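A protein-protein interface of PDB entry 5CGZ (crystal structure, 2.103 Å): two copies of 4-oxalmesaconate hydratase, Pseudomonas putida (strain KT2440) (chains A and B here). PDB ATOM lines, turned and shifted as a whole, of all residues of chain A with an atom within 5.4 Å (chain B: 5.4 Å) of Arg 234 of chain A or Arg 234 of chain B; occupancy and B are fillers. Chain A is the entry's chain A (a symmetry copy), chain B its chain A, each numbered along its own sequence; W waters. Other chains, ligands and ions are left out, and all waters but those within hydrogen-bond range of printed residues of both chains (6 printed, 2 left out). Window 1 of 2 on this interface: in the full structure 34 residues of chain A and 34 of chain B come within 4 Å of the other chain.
NH2 of Arg 234 of chain A lies within hydrogen-bond range of OH of Tyr 155 of chain B, 3.5 Å away.
The side-chain hydroxyl (OH) of Tyr 155 of chain B lies within hydrogen-bond range of the backbone carbonyl oxygen (O) of Leu 239 of chain A, at 2.6 Å.
The backbone carbonyl oxygen (O) of Asp 170 of chain B sits at hydrogen-bond distance from the backbone NH (N) of Arg 234 of chain A (3.0 Å).
The backbone NH (N) of Phe 172 of chain B is in hydrogen-bond range of the backbone carbonyl oxygen (O) of Arg 234 of chain A (2.8 Å).
The backbone NH (N) of Thr 236 of chain A sits at hydrogen-bond distance from the backbone carbonyl oxygen (O) of Phe 172 of chain B (2.8 Å).
The side-chain hydroxyl (OH) of Tyr 155 of chain A sits at hydrogen-bond distance from the guanidinium group (NH2) of Arg 234 of chain B, 3.5 Å away.
The backbone NH (N) of Arg 234 of chain B lies within hydrogen-bond range of the backbone carbonyl oxygen (O) of Asp 170 of chain A (3.0 Å).
N of Phe 172 of chain A sits at hydrogen-bond distance from O of Arg 234 of chain B, 2.8 Å away.
The backbone carbonyl oxygen (O) of Phe 172 of chain A lies within hydrogen-bond range of the backbone NH (N) of Thr 236 of chain B, at 2.8 Å.
OH of Tyr 155 of chain A lies within hydrogen-bond range of O of Leu 239 of chain B, at 2.6 Å.
The side-chain hydroxyl (OG) of Ser 230 of chain B is in hydrogen-bond range of the side-chain hydroxyl (OG1) of Thr 171 of chain B (3.5 Å).
N of Asn 238 of chain B sits at hydrogen-bond distance from OG1 of Thr 236 of chain B, at 3.1 Å.
OD1 of Asp 170 of chain A is in hydrogen-bond range of OG1 of Thr 171 of chain A (2.8 Å).
OD1 of Asp 170 of chain A lies within hydrogen-bond range of OG of Ser 230 of chain A, at 2.7 Å.
The side-chain hydroxyl of Thr 171 of chain A sits at hydrogen-bond distance from the side-chain hydroxyl of Ser 230 of chain A (3.5 Å).
The side-chain hydroxyl (OG1) of Thr 236 of chain A is in hydrogen-bond range of the backbone NH (N) of Asn 238 of chain A.
Pro 233 of chain B touches Asp 170 of chain A (CA to O, 3.3 Å).
Leu 239 of chain B touches Thr 171 of chain A (CD2 to CG2, 3.9 Å).
Phe 172 of chain A touches Val 235 of chain B (O to CA, 3.4 Å).
O of Asp 170 of chain B touches CA of Pro 233 of chain A, 3.3 Å away.
CG of Pro 233 of chain A touches CE2 of Phe 172 of chain B, at 3.7 Å.
O of Arg 234 of chain A touches CA of Thr 171 of chain B, at 3.4 Å.
NE of Arg 234 of chain A touches CD of Arg 234 of chain B, at 3.7 Å.
Phe 172 of chain B touches Val 235 of chain A (O to CA, 3.4 Å).
CG2 of Thr 236 of chain A touches CG2 of Thr 171 of chain B, at 3.8 Å.
Leu 239 of chain A touches Thr 171 of chain B.
Printed residues of chain B within 4 Å of Arg 234 of chain A: Tyr 155 (3.5 Å), Asp 170 (3.0 Å), Thr 171 (3.4 Å), Phe 172 (2.8 Å) and Arg 234 (3.7 Å).
Of the printed residues of chain A, Asp 170 of chain B touches Pro 233 and Arg 234.
Printed residues of chain A within 4 Å of Pro 233 of chain B: Asp 170 and Phe 172.
Printed residues of chain B within 4 Å of Pro 233 of chain A: Asp 170 and Phe 172.
Of the printed residues of chain B, Asp 170 of chain A touches Pro 233 (3.3 Å) and Arg 234 (3.0 Å).
Phe 232 of chain B touches none of the printed residues of chain A.
The nearest residue of chain A that does not touch Arg 234 of chain B is Ser 230 of chain A (5.3 Å).
Hydrophobic or aromatic side chains of chain A that line the printed part of chain B: Tyr 155, Phe 172, Pro 233, Val 235 and Leu 239.
Along chain A the printed residues that touch a printed residue of chain B span positions 155 to 239.
Hydrophobic or aromatic side chains of chain B within 4 Å of the printed part of chain A: Tyr 155, Phe 172, Pro 233, Val 235 and Leu 239.
Along chain B the printed residues that touch a printed residue of chain A span positions 155 to 239.
Among the printed residues, 23 pairs touch across the chains.
Asp 170 of chain A touches Arg 234 of chain B, and with the chains exchanged Arg 234 of chain A touches Asp 170 of chain B.
Thr 171 of chain A touches Thr 236 of chain B, and with the chains exchanged Thr 236 of chain A touches Thr 171 of chain B.
Phe 172 of chain A touches Pro 233 of chain B, and with the chains exchanged Pro 233 of chain A touches Phe 172 of chain B.
Arg 234 of chain B touches its own counterpart, Arg 234 of chain A.
Positions printed for both chains: 155, 170, 171, 172, 230, 232, 233, 234, 235, 236, 238, 239 and 240.
Of the 23 pairs that touch across the chains among the printed residues, 23 have their exchanged pair printed and touching as well.
Water W5 bridges OH of Tyr 155 of chain B and NH2 of Arg 234 of chain A.
Water W4 bridges the side-chain hydroxyl (OH) of Tyr 155 of chain A (2.6 Å) and the guanidinium group (NH2) of Arg 234 of chain B (3.4 Å).
Water W1 lies within hydrogen-bond range of OG of Ser 230 of chain A (2.8 Å), NH2 of Arg 234 of chain B (3.1 Å) and OG1 of Thr 171 of chain A (3.3 Å).
Water W6 lies within hydrogen-bond range of OG of Ser 230 of chain B, NH2 of Arg 234 of chain A and OG1 of Thr 171 of chain B.
Water W2 bridges the backbone carbonyl oxygen of Asp 170 of chain B (3.1 Å) and the backbone carbonyl oxygen of Phe 232 of chain A (3.4 Å).
Water W3 bridges the backbone carbonyl oxygen of Asp 170 of chain A (3.1 Å) and the backbone carbonyl oxygen of Phe 232 of chain B (3.4 Å).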
ATOM      1  N   TYR A 155     -14.677  -2.887 -18.123  1.00  0.00           N
ATOM      2  CA  TYR A 155     -13.329  -2.335 -18.211  1.00  0.00           C
ATOM      3  C   TYR A 155     -12.943  -1.651 -16.920  1.00  0.00           C
ATOM      4  O   TYR A 155     -13.775  -1.001 -16.291  1.00  0.00           O
ATOM      5  CB  TYR A 155     -13.212  -1.301 -19.335  1.00  0.00           C
ATOM      6  CG  TYR A 155     -13.616  -1.754 -20.720  1.00  0.00           C
ATOM      7  CD1 TYR A 155     -14.942  -1.659 -21.140  1.00  0.00           C
ATOM      8  CD2 TYR A 155     -12.669  -2.228 -21.624  1.00  0.00           C
ATOM      9  CE1 TYR A 155     -15.320  -2.051 -22.415  1.00  0.00           C
ATOM     10  CE2 TYR A 155     -13.035  -2.621 -22.914  1.00  0.00           C
ATOM     11  CZ  TYR A 155     -14.368  -2.525 -23.299  1.00  0.00           C
ATOM     12  OH  TYR A 155     -14.761  -2.897 -24.569  1.00  0.00           O
ATOM     13  N   ASP A 170      -5.201  -2.404 -22.205  1.00  0.00           N
ATOM     14  CA  ASP A 170      -5.190  -3.197 -23.436  1.00  0.00           C
ATOM     15  C   ASP A 170      -6.081  -2.514 -24.481  1.00  0.00           C
ATOM     16  O   ASP A 170      -6.193  -2.965 -25.625  1.00  0.00           O
ATOM     17  CB  ASP A 170      -5.654  -4.640 -23.178  1.00  0.00           C
ATOM     18  CG  ASP A 170      -7.047  -4.712 -22.538  1.00  0.00           C
ATOM     19  OD1 ASP A 170      -7.975  -4.022 -22.996  1.00  0.00           O
ATOM     20  OD2 ASP A 170      -7.217  -5.460 -21.564  1.00  0.00           O
ATOM     21  N   THR A 171      -6.702  -1.411 -24.077  1.00  0.00           N
ATOM     22  CA  THR A 171      -7.620  -0.677 -24.951  1.00  0.00           C
ATOM     23  C   THR A 171      -7.419   0.822 -24.756  1.00  0.00           C
ATOM     24  O   THR A 171      -7.469   1.306 -23.632  1.00  0.00           O
ATOM     25  CB  THR A 171      -9.094  -1.050 -24.655  1.00  0.00           C
ATOM     26  OG1 THR A 171      -9.279  -2.456 -24.843  1.00  0.00           O
ATOM     27  CG2 THR A 171     -10.075  -0.291 -25.571  1.00  0.00           C
ATOM     28  N   PHE A 172      -7.158   1.552 -25.839  1.00  0.00           N
ATOM     29  CA  PHE A 172      -7.133   3.015 -25.775  1.00  0.00           C
ATOM     30  C   PHE A 172      -8.348   3.598 -26.471  1.00  0.00           C
ATOM     31  O   PHE A 172      -8.624   3.295 -27.639  1.00  0.00           O
ATOM     32  CB  PHE A 172      -5.862   3.598 -26.412  1.00  0.00           C
ATOM     33  CG  PHE A 172      -4.623   3.394 -25.594  1.00  0.00           C
ATOM     34  CD1 PHE A 172      -4.482   4.019 -24.365  1.00  0.00           C
ATOM     35  CD2 PHE A 172      -3.592   2.592 -26.061  1.00  0.00           C
ATOM     36  CE1 PHE A 172      -3.333   3.834 -23.598  1.00  0.00           C
ATOM     37  CE2 PHE A 172      -2.439   2.406 -25.311  1.00  0.00           C
ATOM     38  CZ  PHE A 172      -2.312   3.025 -24.072  1.00  0.00           C
ATOM     39  N   SER A 230      -9.546  -4.467 -20.100  1.00  0.00           N
ATOM     40  CA  SER A 230     -10.714  -5.317 -20.301  1.00  0.00           C
ATOM     41  C   SER A 230     -10.756  -6.487 -19.354  1.00  0.00           C
ATOM     42  O   SER A 230      -9.747  -7.141 -19.128  1.00  0.00           O
ATOM     43  CB  SER A 230     -10.734  -5.865 -21.730  1.00  0.00           C
ATOM     44  OG  SER A 230     -10.543  -4.814 -22.655  1.00  0.00           O
ATOM     45  N   PHE A 232     -13.091  -9.104 -19.925  1.00  0.00           N
ATOM     46  CA  PHE A 232     -13.473 -10.270 -20.714  1.00  0.00           C
ATOM     47  C   PHE A 232     -12.897 -10.229 -22.124  1.00  0.00           C
ATOM     48  O   PHE A 232     -12.642  -9.150 -22.666  1.00  0.00           O
ATOM     49  CB  PHE A 232     -15.003 -10.389 -20.803  1.00  0.00           C
ATOM     50  CG  PHE A 232     -15.675 -10.468 -19.469  1.00  0.00           C
ATOM     51  CD1 PHE A 232     -15.653 -11.650 -18.740  1.00  0.00           C
ATOM     52  CD2 PHE A 232     -16.314  -9.357 -18.935  1.00  0.00           C
ATOM     53  CE1 PHE A 232     -16.259 -11.729 -17.496  1.00  0.00           C
ATOM     54  CE2 PHE A 232     -16.926  -9.419 -17.683  1.00  0.00           C
ATOM     55  CZ  PHE A 232     -16.895 -10.601 -16.961  1.00  0.00           C
ATOM     56  N   PRO A 233     -12.719 -11.411 -22.732  1.00  0.00           N
ATOM     57  CA  PRO A 233     -12.333 -11.488 -24.143  1.00  0.00           C
ATOM     58  C   PRO A 233     -13.403 -10.854 -25.027  1.00  0.00           C
ATOM     59  O   PRO A 233     -14.595 -11.062 -24.797  1.00  0.00           O
ATOM     60  CB  PRO A 233     -12.233 -12.996 -24.397  1.00  0.00           C
ATOM     61  CG  PRO A 233     -13.164 -13.609 -23.367  1.00  0.00           C
ATOM     62  CD  PRO A 233     -13.003 -12.741 -22.151  1.00  0.00           C
ATOM     63  N   ARG A 234     -12.998 -10.088 -26.028  1.00  0.00           N
ATOM     64  CA  ARG A 234     -13.980  -9.511 -26.932  1.00  0.00           C
ATOM     65  C   ARG A 234     -14.251 -10.480 -28.086  1.00  0.00           C
ATOM     66  O   ARG A 234     -13.432 -11.345 -28.382  1.00  0.00           O
ATOM     67  CB  ARG A 234     -13.501  -8.159 -27.463  1.00  0.00           C
ATOM     68  CG  ARG A 234     -12.325  -8.273 -28.393  1.00  0.00           C
ATOM     69  CD  ARG A 234     -11.800  -6.898 -28.816  1.00  0.00           C
ATOM     70  NE  ARG A 234     -10.633  -7.054 -29.679  1.00  0.00           N
ATOM     71  CZ  ARG A 234     -10.619  -6.778 -30.979  1.00  0.00           C
ATOM     72  NH1 ARG A 234     -11.711  -6.314 -31.575  1.00  0.00           N
ATOM     73  NH2 ARG A 234      -9.507  -6.964 -31.680  1.00  0.00           N
ATOM     74  N   VAL A 235     -15.413 -10.334 -28.716  1.00  0.00           N
ATOM     75  CA  VAL A 235     -15.822 -11.189 -29.822  1.00  0.00           C
ATOM     76  C   VAL A 235     -15.967 -10.332 -31.066  1.00  0.00           C
ATOM     77  O   VAL A 235     -16.633  -9.299 -31.031  1.00  0.00           O
ATOM     78  CB  VAL A 235     -17.154 -11.899 -29.535  1.00  0.00           C
ATOM     79  CG1 VAL A 235     -17.559 -12.777 -30.724  1.00  0.00           C
ATOM     80  CG2 VAL A 235     -17.055 -12.722 -28.256  1.00  0.00           C
ATOM     81  N   THR A 236     -15.349 -10.749 -32.161  1.00  0.00           N
ATOM     82  CA  THR A 236     -15.331  -9.916 -33.354  1.00  0.00           C
ATOM     83  C   THR A 236     -15.307 -10.737 -34.642  1.00  0.00           C
ATOM     84  O   THR A 236     -15.116 -11.960 -34.619  1.00  0.00           O
ATOM     85  CB  THR A 236     -14.104  -8.971 -33.340  1.00  0.00           C
ATOM     86  OG1 THR A 236     -14.186  -8.069 -34.447  1.00  0.00           O
ATOM     87  CG2 THR A 236     -12.788  -9.768 -33.431  1.00  0.00           C
ATOM     88  N   ASN A 238     -13.441  -9.184 -37.232  1.00  0.00           N
ATOM     89  CA  ASN A 238     -12.344  -8.545 -37.945  1.00  0.00           C
ATOM     90  C   ASN A 238     -11.188  -8.194 -37.021  1.00  0.00           C
ATOM     91  O   ASN A 238     -11.401  -7.639 -35.946  1.00  0.00           O
ATOM     92  CB  ASN A 238     -12.848  -7.293 -38.669  1.00  0.00           C
ATOM     93  CG  ASN A 238     -11.732  -6.555 -39.395  1.00  0.00           C
ATOM     94  OD1 ASN A 238     -11.039  -5.724 -38.808  1.00  0.00           O
ATOM     95  ND2 ASN A 238     -11.544  -6.872 -40.670  1.00  0.00           N
ATOM     96  N   LEU A 239      -9.966  -8.495 -37.457  1.00  0.00           N
ATOM     97  CA  LEU A 239      -8.797  -8.394 -36.578  1.00  0.00           C
ATOM     98  C   LEU A 239      -7.951  -7.142 -36.779  1.00  0.00           C
ATOM     99  O   LEU A 239      -6.916  -6.998 -36.135  1.00  0.00           O
ATOM    100  CB  LEU A 239      -7.904  -9.632 -36.748  1.00  0.00           C
ATOM    101  CG  LEU A 239      -8.545 -10.933 -36.251  1.00  0.00           C
ATOM    102  CD1 LEU A 239      -7.637 -12.124 -36.499  1.00  0.00           C
ATOM    103  CD2 LEU A 239      -8.935 -10.840 -34.767  1.00  0.00           C
ATOM    104  N   ALA A 240      -8.378  -6.233 -37.653  1.00  0.00           N
ATOM    105  CA  ALA A 240      -7.597  -5.016 -37.902  1.00  0.00           C
ATOM    106  C   ALA A 240      -7.647  -4.072 -36.697  1.00  0.00           C
ATOM    107  O   ALA A 240      -6.819  -3.162 -36.558  1.00  0.00           O
ATOM    108  CB  ALA A 240      -8.093  -4.301 -39.150  1.00  0.00           C
ATOM    109  OXT ALA A 240      -8.530  -4.207 -35.840  1.00  0.00           O
ATOM    110  N   TYR B 155      -1.199 -10.926 -33.327  1.00  0.00           N
ATOM    111  CA  TYR B 155      -1.920 -11.868 -32.478  1.00  0.00           C
ATOM    112  C   TYR B 155      -1.237 -13.217 -32.470  1.00  0.00           C
ATOM    113  O   TYR B 155      -0.734 -13.662 -33.499  1.00  0.00           O
ATOM    114  CB  TYR B 155      -3.358 -12.081 -32.959  1.00  0.00           C
ATOM    115  CG  TYR B 155      -4.215 -10.844 -33.107  1.00  0.00           C
ATOM    116  CD1 TYR B 155      -4.213 -10.116 -34.295  1.00  0.00           C
ATOM    117  CD2 TYR B 155      -5.062 -10.432 -32.080  1.00  0.00           C
ATOM    118  CE1 TYR B 155      -5.011  -8.992 -34.450  1.00  0.00           C
ATOM    119  CE2 TYR B 155      -5.877  -9.306 -32.225  1.00  0.00           C
ATOM    120  CZ  TYR B 155      -5.843  -8.593 -33.419  1.00  0.00           C
ATOM    121  OH  TYR B 155      -6.641  -7.482 -33.596  1.00  0.00           O
ATOM    122  N   ASP B 170      -7.730 -13.239 -25.667  1.00  0.00           N
ATOM    123  CA  ASP B 170      -8.434 -12.016 -25.278  1.00  0.00           C
ATOM    124  C   ASP B 170      -9.349 -11.576 -26.428  1.00  0.00           C
ATOM    125  O   ASP B 170     -10.091 -10.595 -26.321  1.00  0.00           O
ATOM    126  CB  ASP B 170      -7.449 -10.897 -24.902  1.00  0.00           C
ATOM    127  CG  ASP B 170      -6.454 -10.578 -26.026  1.00  0.00           C
ATOM    128  OD1 ASP B 170      -6.863 -10.437 -27.193  1.00  0.00           O
ATOM    129  OD2 ASP B 170      -5.251 -10.471 -25.745  1.00  0.00           O
ATOM    130  N   THR B 171      -9.298 -12.325 -27.524  1.00  0.00           N
ATOM    131  CA  THR B 171     -10.082 -12.001 -28.718  1.00  0.00           C
ATOM    132  C   THR B 171     -10.628 -13.286 -29.332  1.00  0.00           C
ATOM    133  O   THR B 171      -9.868 -14.211 -29.595  1.00  0.00           O
ATOM    134  CB  THR B 171      -9.224 -11.245 -29.763  1.00  0.00           C
ATOM    135  OG1 THR B 171      -8.717 -10.039 -29.184  1.00  0.00           O
ATOM    136  CG2 THR B 171     -10.036 -10.890 -31.025  1.00  0.00           C
ATOM    137  N   PHE B 172     -11.943 -13.360 -29.531  1.00  0.00           N
ATOM    138  CA  PHE B 172     -12.532 -14.473 -30.279  1.00  0.00           C
ATOM    139  C   PHE B 172     -13.009 -14.004 -31.640  1.00  0.00           C
ATOM    140  O   PHE B 172     -13.786 -13.046 -31.751  1.00  0.00           O
ATOM    141  CB  PHE B 172     -13.709 -15.115 -29.528  1.00  0.00           C
ATOM    142  CG  PHE B 172     -13.299 -15.935 -28.343  1.00  0.00           C
ATOM    143  CD1 PHE B 172     -12.569 -17.102 -28.514  1.00  0.00           C
ATOM    144  CD2 PHE B 172     -13.658 -15.551 -27.059  1.00  0.00           C
ATOM    145  CE1 PHE B 172     -12.184 -17.870 -27.417  1.00  0.00           C
ATOM    146  CE2 PHE B 172     -13.288 -16.312 -25.959  1.00  0.00           C
ATOM    147  CZ  PHE B 172     -12.543 -17.473 -26.139  1.00  0.00           C
ATOM    148  N   SER B 230      -3.737 -10.958 -28.201  1.00  0.00           N
ATOM    149  CA  SER B 230      -3.186  -9.723 -28.750  1.00  0.00           C
ATOM    150  C   SER B 230      -1.862  -9.351 -28.138  1.00  0.00           C
ATOM    151  O   SER B 230      -1.690  -9.431 -26.930  1.00  0.00           O
ATOM    152  CB  SER B 230      -4.156  -8.561 -28.523  1.00  0.00           C
ATOM    153  OG  SER B 230      -5.455  -8.923 -28.944  1.00  0.00           O
ATOM    154  N   PHE B 232      -0.507  -6.126 -28.757  1.00  0.00           N
ATOM    155  CA  PHE B 232      -0.555  -4.692 -28.491  1.00  0.00           C
ATOM    156  C   PHE B 232      -1.944  -4.228 -28.068  1.00  0.00           C
ATOM    157  O   PHE B 232      -2.949  -4.840 -28.438  1.00  0.00           O
ATOM    158  CB  PHE B 232      -0.118  -3.894 -29.730  1.00  0.00           C
ATOM    159  CG  PHE B 232       1.252  -4.248 -30.217  1.00  0.00           C
ATOM    160  CD1 PHE B 232       2.377  -3.779 -29.552  1.00  0.00           C
ATOM    161  CD2 PHE B 232       1.415  -5.063 -31.328  1.00  0.00           C
ATOM    162  CE1 PHE B 232       3.650  -4.115 -29.984  1.00  0.00           C
ATOM    163  CE2 PHE B 232       2.689  -5.413 -31.776  1.00  0.00           C
ATOM    164  CZ  PHE B 232       3.806  -4.945 -31.103  1.00  0.00           C
ATOM    165  N   PRO B 233      -2.000  -3.122 -27.312  1.00  0.00           N
ATOM    166  CA  PRO B 233      -3.280  -2.488 -26.988  1.00  0.00           C
ATOM    167  C   PRO B 233      -3.984  -2.020 -28.260  1.00  0.00           C
ATOM    168  O   PRO B 233      -3.339  -1.472 -29.154  1.00  0.00           O
ATOM    169  CB  PRO B 233      -2.871  -1.297 -26.116  1.00  0.00           C
ATOM    170  CG  PRO B 233      -1.451  -0.988 -26.551  1.00  0.00           C
ATOM    171  CD  PRO B 233      -0.844  -2.334 -26.833  1.00  0.00           C
ATOM    172  N   ARG B 234      -5.287  -2.227 -28.351  1.00  0.00           N
ATOM    173  CA  ARG B 234      -6.010  -1.745 -29.517  1.00  0.00           C
ATOM    174  C   ARG B 234      -6.487  -0.311 -29.273  1.00  0.00           C
ATOM    175  O   ARG B 234      -6.610   0.121 -28.130  1.00  0.00           O
ATOM    176  CB  ARG B 234      -7.192  -2.659 -29.841  1.00  0.00           C
ATOM    177  CG  ARG B 234      -8.286  -2.596 -28.812  1.00  0.00           C
ATOM    178  CD  ARG B 234      -9.401  -3.605 -29.105  1.00  0.00           C
ATOM    179  NE  ARG B 234     -10.418  -3.542 -28.059  1.00  0.00           N
ATOM    180  CZ  ARG B 234     -11.645  -3.065 -28.234  1.00  0.00           C
ATOM    181  NH1 ARG B 234     -12.023  -2.614 -29.426  1.00  0.00           N
ATOM    182  NH2 ARG B 234     -12.495  -3.041 -27.215  1.00  0.00           N
ATOM    183  N   VAL B 235      -6.735   0.420 -30.356  1.00  0.00           N
ATOM    184  CA  VAL B 235      -7.179   1.806 -30.287  1.00  0.00           C
ATOM    185  C   VAL B 235      -8.564   1.898 -30.902  1.00  0.00           C
ATOM    186  O   VAL B 235      -8.781   1.416 -32.011  1.00  0.00           O
ATOM    187  CB  VAL B 235      -6.225   2.750 -31.034  1.00  0.00           C
ATOM    188  CG1 VAL B 235      -6.732   4.195 -30.952  1.00  0.00           C
ATOM    189  CG2 VAL B 235      -4.812   2.633 -30.476  1.00  0.00           C
ATOM    190  N   THR B 236      -9.498   2.513 -30.191  1.00  0.00           N
ATOM    191  CA  THR B 236     -10.878   2.527 -30.654  1.00  0.00           C
ATOM    192  C   THR B 236     -11.622   3.795 -30.240  1.00  0.00           C
ATOM    193  O   THR B 236     -11.129   4.593 -29.432  1.00  0.00           O
ATOM    194  CB  THR B 236     -11.647   1.297 -30.110  1.00  0.00           C
ATOM    195  OG1 THR B 236     -12.953   1.258 -30.690  1.00  0.00           O
ATOM    196  CG2 THR B 236     -11.774   1.355 -28.575  1.00  0.00           C
ATOM    197  N   ASN B 238     -15.058   3.218 -29.557  1.00  0.00           N
ATOM    198  CA  ASN B 238     -16.271   2.651 -28.986  1.00  0.00           C
ATOM    199  C   ASN B 238     -15.987   1.405 -28.161  1.00  0.00           C
ATOM    200  O   ASN B 238     -15.252   0.525 -28.600  1.00  0.00           O
ATOM    201  CB  ASN B 238     -17.277   2.338 -30.097  1.00  0.00           C
ATOM    202  CG  ASN B 238     -18.550   1.698 -29.562  1.00  0.00           C
ATOM    203  OD1 ASN B 238     -18.622   0.480 -29.393  1.00  0.00           O
ATOM    204  ND2 ASN B 238     -19.551   2.520 -29.276  1.00  0.00           N
ATOM    205  N   LEU B 239     -16.595   1.324 -26.979  1.00  0.00           N
ATOM    206  CA  LEU B 239     -16.245   0.279 -26.011  1.00  0.00           C
ATOM    207  C   LEU B 239     -17.215  -0.896 -25.960  1.00  0.00           C
ATOM    208  O   LEU B 239     -17.042  -1.791 -25.137  1.00  0.00           O
ATOM    209  CB  LEU B 239     -16.121   0.885 -24.605  1.00  0.00           C
ATOM    210  CG  LEU B 239     -14.941   1.851 -24.448  1.00  0.00           C
ATOM    211  CD1 LEU B 239     -14.908   2.457 -23.056  1.00  0.00           C
ATOM    212  CD2 LEU B 239     -13.605   1.170 -24.781  1.00  0.00           C
ATOM    213  N   ALA B 240     -18.222  -0.913 -26.831  1.00  0.00           N
ATOM    214  CA  ALA B 240     -19.197  -2.009 -26.817  1.00  0.00           C
ATOM    215  C   ALA B 240     -18.570  -3.312 -27.320  1.00  0.00           C
ATOM    216  O   ALA B 240     -19.097  -4.410 -27.092  1.00  0.00           O
ATOM    217  CB  ALA B 240     -20.418  -1.657 -27.655  1.00  0.00           C
ATOM    218  OXT ALA B 240     -17.518  -3.283 -27.971  1.00  0.00           O
HETATM  219  O   HOH W   1     -11.148  -5.086 -25.340  1.00  0.00           O
HETATM  220  O   HOH W   2     -10.153  -7.990 -24.599  1.00  0.00           O
HETATM  221  O   HOH W   3      -5.844  -5.748 -26.999  1.00  0.00           O
HETATM  222  O   HOH W   4     -14.348  -5.353 -25.459  1.00  0.00           O
HETATM  223  O   HOH W   5      -6.455  -5.398 -31.978  1.00  0.00           O
HETATM  224  O   HOH W   6      -7.434  -7.045 -29.399  1.00  0.00           O
